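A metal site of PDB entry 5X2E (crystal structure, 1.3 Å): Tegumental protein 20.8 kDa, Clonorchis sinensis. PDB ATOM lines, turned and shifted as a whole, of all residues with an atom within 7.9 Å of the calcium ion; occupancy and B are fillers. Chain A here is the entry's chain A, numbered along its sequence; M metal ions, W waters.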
ATOM      1  N   PHE A   7     -16.140 -10.426   9.364  1.00  0.00           N
ATOM      2  CA  PHE A   7     -14.844 -10.888   9.895  1.00  0.00           C
ATOM      3  C   PHE A   7     -14.200  -9.741  10.694  1.00  0.00           C
ATOM      4  O   PHE A   7     -13.745  -9.937  11.822  1.00  0.00           O
ATOM      5  CB  PHE A   7     -13.864 -11.313   8.797  1.00  0.00           C
ATOM      6  CG  PHE A   7     -12.589 -11.850   9.354  1.00  0.00           C
ATOM      7  CD1 PHE A   7     -12.416 -13.214   9.499  1.00  0.00           C
ATOM      8  CD2 PHE A   7     -11.538 -10.992   9.728  1.00  0.00           C
ATOM      9  CE1 PHE A   7     -11.262 -13.739  10.055  1.00  0.00           C
ATOM     10  CE2 PHE A   7     -10.382 -11.513  10.300  1.00  0.00           C
ATOM     11  CZ  PHE A   7     -10.247 -12.879  10.450  1.00  0.00           C
ATOM     12  N   ILE A  10     -16.041  -9.125  14.010  1.00  0.00           N
ATOM     13  CA  ILE A  10     -15.793 -10.128  15.041  1.00  0.00           C
ATOM     14  C   ILE A  10     -14.365  -9.986  15.617  1.00  0.00           C
ATOM     15  O   ILE A  10     -14.171 -10.078  16.832  1.00  0.00           O
ATOM     16  CB  ILE A  10     -16.011 -11.544  14.484  1.00  0.00           C
ATOM     17  CG1 ILE A  10     -17.478 -11.745  14.076  1.00  0.00           C
ATOM     18  CG2 ILE A  10     -15.588 -12.579  15.522  1.00  0.00           C
ATOM     19  CD1 ILE A  10     -17.693 -13.007  13.239  1.00  0.00           C
ATOM     20  N   ASP A  11     -13.401  -9.758  14.745  1.00  0.00           N
ATOM     21  CA  ASP A  11     -11.993  -9.727  15.092  1.00  0.00           C
ATOM     22  C   ASP A  11     -11.634  -8.357  15.638  1.00  0.00           C
ATOM     23  O   ASP A  11     -10.901  -7.561  15.013  1.00  0.00           O
ATOM     24  CB  ASP A  11     -11.137 -10.081  13.884  1.00  0.00           C
ATOM     25  CG  ASP A  11      -9.680 -10.080  14.202  1.00  0.00           C
ATOM     26  OD1 ASP A  11      -9.305 -10.453  15.337  1.00  0.00           O
ATOM     27  OD2 ASP A  11      -8.901  -9.652  13.317  1.00  0.00           O
ATOM     28  N   LYS A  12     -12.156  -8.067  16.820  1.00  0.00           N
ATOM     29  CA  LYS A  12     -12.155  -6.704  17.329  1.00  0.00           C
ATOM     30  C   LYS A  12     -10.764  -6.198  17.687  1.00  0.00           C
ATOM     31  O   LYS A  12     -10.543  -5.004  17.729  1.00  0.00           O
ATOM     32  CB  LYS A  12     -13.062  -6.608  18.548  1.00  0.00           C
ATOM     33  CG  LYS A  12     -12.723  -7.603  19.604  1.00  0.00           C
ATOM     34  CD  LYS A  12     -13.724  -7.536  20.727  1.00  0.00           C
ATOM     35  CE  LYS A  12     -13.124  -8.111  21.962  1.00  0.00           C
ATOM     36  NZ  LYS A  12     -13.861  -7.652  23.163  1.00  0.00           N
ATOM     37  N   ASP A  13      -9.815  -7.112  17.955  1.00  0.00           N
ATOM     38  CA  ASP A  13      -8.454  -6.676  18.262  1.00  0.00           C
ATOM     39  C   ASP A  13      -7.537  -6.636  17.040  1.00  0.00           C
ATOM     40  O   ASP A  13      -6.362  -6.283  17.147  1.00  0.00           O
ATOM     41  CB  ASP A  13      -7.838  -7.510  19.375  1.00  0.00           C
ATOM     42  CG  ASP A  13      -7.718  -8.960  19.016  1.00  0.00           C
ATOM     43  OD1 ASP A  13      -7.985  -9.383  17.856  1.00  0.00           O
ATOM     44  OD2 ASP A  13      -7.308  -9.713  19.919  1.00  0.00           O
ATOM     45  N   GLY A  14      -8.075  -6.923  15.847  1.00  0.00           N
ATOM     46  CA  GLY A  14      -7.292  -6.791  14.636  1.00  0.00           C
ATOM     47  C   GLY A  14      -6.191  -7.827  14.463  1.00  0.00           C
ATOM     48  O   GLY A  14      -5.318  -7.635  13.610  1.00  0.00           O
ATOM     49  N   THR A  15      -6.207  -8.935  15.207  1.00  0.00           N
ATOM     50  CA  THR A  15      -5.093  -9.880  15.060  1.00  0.00           C
ATOM     51  C   THR A  15      -5.221 -10.753  13.814  1.00  0.00           C
ATOM     52  O   THR A  15      -4.285 -11.497  13.497  1.00  0.00           O
ATOM     53  CB  THR A  15      -4.976 -10.803  16.289  1.00  0.00           C
ATOM     54  OG1 THR A  15      -6.199 -11.566  16.436  1.00  0.00           O
ATOM     55  CG2 THR A  15      -4.687  -9.986  17.560  1.00  0.00           C
ATOM     56  N   ASN A  16      -6.370 -10.683  13.142  1.00  0.00           N
ATOM     57  CA  ASN A  16      -6.667 -11.572  12.009  1.00  0.00           C
ATOM     58  C   ASN A  16      -6.730 -13.048  12.396  1.00  0.00           C
ATOM     59  O   ASN A  16      -6.649 -13.949  11.551  1.00  0.00           O
ATOM     60  CB  ASN A  16      -5.679 -11.349  10.862  1.00  0.00           C
ATOM     61  CG  ASN A  16      -5.782  -9.965  10.311  1.00  0.00           C
ATOM     62  OD1 ASN A  16      -6.866  -9.531   9.918  1.00  0.00           O
ATOM     63  ND2 ASN A  16      -4.675  -9.222  10.336  1.00  0.00           N
ATOM     64  N   VAL A  17      -6.961 -13.270  13.681  1.00  0.00           N
ATOM     65  CA  VAL A  17      -7.385 -14.540  14.209  1.00  0.00           C
ATOM     66  C   VAL A  17      -8.642 -14.266  15.032  1.00  0.00           C
ATOM     67  O   VAL A  17      -8.594 -13.473  15.983  1.00  0.00           O
ATOM     68  CB  VAL A  17      -6.316 -15.197  15.072  1.00  0.00           C
ATOM     69  CG1 VAL A  17      -6.821 -16.559  15.546  1.00  0.00           C
ATOM     70  CG2 VAL A  17      -4.997 -15.338  14.306  1.00  0.00           C
ATOM     71  N   ILE A  18      -9.747 -14.904  14.673  1.00  0.00           N
ATOM     72  CA  ILE A  18     -10.966 -14.854  15.449  1.00  0.00           C
ATOM     73  C   ILE A  18     -10.852 -15.898  16.563  1.00  0.00           C
ATOM     74  O   ILE A  18     -10.733 -17.112  16.335  1.00  0.00           O
ATOM     75  CB  ILE A  18     -12.203 -15.081  14.563  1.00  0.00           C
ATOM     76  CG1 ILE A  18     -12.452 -13.826  13.718  1.00  0.00           C
ATOM     77  CG2 ILE A  18     -13.410 -15.486  15.435  1.00  0.00           C
ATOM     78  CD1 ILE A  18     -13.633 -13.999  12.730  1.00  0.00           C
ATOM     79  N   SER A  19     -10.841 -15.424  17.794  1.00  0.00           N
ATOM     80  CA  SER A  19     -10.862 -16.326  18.908  1.00  0.00           C
ATOM     81  C   SER A  19     -12.282 -16.817  19.151  1.00  0.00           C
ATOM     82  O   SER A  19     -13.280 -16.162  18.775  1.00  0.00           O
ATOM     83  CB  SER A  19     -10.318 -15.619  20.176  1.00  0.00           C
ATOM     84  OG  SER A  19     -11.313 -14.724  20.662  1.00  0.00           O
ATOM     85  N   TYR A  20     -12.422 -17.959  19.815  1.00  0.00           N
ATOM     86  CA  TYR A  20     -13.745 -18.432  20.132  1.00  0.00           C
ATOM     87  C   TYR A  20     -14.533 -17.439  21.044  1.00  0.00           C
ATOM     88  O   TYR A  20     -15.691 -17.152  20.764  1.00  0.00           O
ATOM     89  CB  TYR A  20     -13.680 -19.826  20.719  1.00  0.00           C
ATOM     90  CG  TYR A  20     -13.227 -20.952  19.773  1.00  0.00           C
ATOM     91  CD1 TYR A  20     -13.106 -20.768  18.407  1.00  0.00           C
ATOM     92  CD2 TYR A  20     -12.925 -22.205  20.302  1.00  0.00           C
ATOM     93  CE1 TYR A  20     -12.734 -21.834  17.575  1.00  0.00           C
ATOM     94  CE2 TYR A  20     -12.538 -23.247  19.492  1.00  0.00           C
ATOM     95  CZ  TYR A  20     -12.430 -23.059  18.127  1.00  0.00           C
ATOM     96  OH  TYR A  20     -12.053 -24.169  17.364  1.00  0.00           O
ATOM     97  N   GLU A  22     -14.283 -14.153  20.918  1.00  0.00           N
ATOM     98  CA  GLU A  22     -14.699 -13.089  20.010  1.00  0.00           C
ATOM     99  C   GLU A  22     -15.948 -13.499  19.233  1.00  0.00           C
ATOM    100  O   GLU A  22     -16.879 -12.701  19.109  1.00  0.00           O
ATOM    101  CB  GLU A  22     -13.556 -12.757  19.012  1.00  0.00           C
ATOM    102  CG  GLU A  22     -12.491 -11.858  19.608  1.00  0.00           C
ATOM    103  CD  GLU A  22     -11.303 -11.636  18.672  1.00  0.00           C
ATOM    104  OE1 GLU A  22     -11.065 -12.466  17.747  1.00  0.00           O
ATOM    105  OE2 GLU A  22     -10.579 -10.629  18.815  1.00  0.00           O
ATOM    106  N   ILE A  52      -9.926 -19.256  14.488  1.00  0.00           N
ATOM    107  CA  ILE A  52     -10.268 -19.115  13.087  1.00  0.00           C
ATOM    108  C   ILE A  52      -9.360 -18.069  12.468  1.00  0.00           C
ATOM    109  O   ILE A  52      -9.471 -16.886  12.751  1.00  0.00           O
ATOM    110  CB  ILE A  52     -11.750 -18.736  12.910  1.00  0.00           C
ATOM    111  CG1 ILE A  52     -12.685 -19.916  13.306  1.00  0.00           C
ATOM    112  CG2 ILE A  52     -12.003 -18.255  11.481  1.00  0.00           C
ATOM    113  CD1 ILE A  52     -14.115 -19.524  13.573  1.00  0.00           C
ATOM    114  N   ARG A  72     -10.441  -3.221   6.534  1.00  0.00           N
ATOM    115  CA  ARG A  72      -9.970  -2.797   7.827  1.00  0.00           C
ATOM    116  C   ARG A  72      -9.371  -1.404   7.794  1.00  0.00           C
ATOM    117  O   ARG A  72      -9.687  -0.580   8.646  1.00  0.00           O
ATOM    118  CB  ARG A  72      -8.910  -3.791   8.327  1.00  0.00           C
ATOM    119  CG  ARG A  72      -8.309  -3.493   9.713  1.00  0.00           C
ATOM    120  CD  ARG A  72      -8.954  -4.307  10.803  1.00  0.00           C
ATOM    121  NE  ARG A  72      -8.871  -5.747  10.577  1.00  0.00           N
ATOM    122  CZ  ARG A  72      -9.377  -6.655  11.418  1.00  0.00           C
ATOM    123  NH1 ARG A  72     -10.037  -6.243  12.502  1.00  0.00           N
ATOM    124  NH2 ARG A  72      -9.235  -7.965  11.167  1.00  0.00           N
HETATM  125 CA    CA M   1      -8.803 -11.518  17.237  1.00  0.00          CA
HETATM  126  O   HOH W   1      -8.042 -12.818  19.031  1.00  0.00           O
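The side-chain carboxylate (OD1) of Asp 11 is bound to the calcium ion (2.2 Å).
The calcium ion is bound by the backbone carbonyl oxygen (O) of Val 17 (2.3 Å).
Water W1 is bound to the calcium ion (2.3 Å).
The calcium ion is bound by the side-chain carboxylate (OD1) of Asp 13, 2.4 Å away.
The calcium ion is bound by OE1 of Glu 22.
The calcium ion is bound by the side-chain carboxylate (OE2) of Glu 22 (2.5 Å).
OG1 of Thr 15 is bound to the calcium ion, 2.7 Å away.
OD2 of Asp 11 is in salt-bridge range of NH2 of Arg 72, at 2.8 Å.
The side-chain hydroxyl (OG) of Ser 19 is in hydrogen-bond range of the backbone NH (N) of Glu 22, 3.0 Å away.
The backbone NH of Asn 16 sits at hydrogen-bond distance from the side-chain carboxylate of Asp 11 (2.7 Å).
Five residues have an atom within 4 Å of the calcium ion: Asp 11, Asp 13, Thr 15, Val 17 and Glu 22.
The nearest printed residue that does not touch the calcium ion is Ile 18 (4.4 Å).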
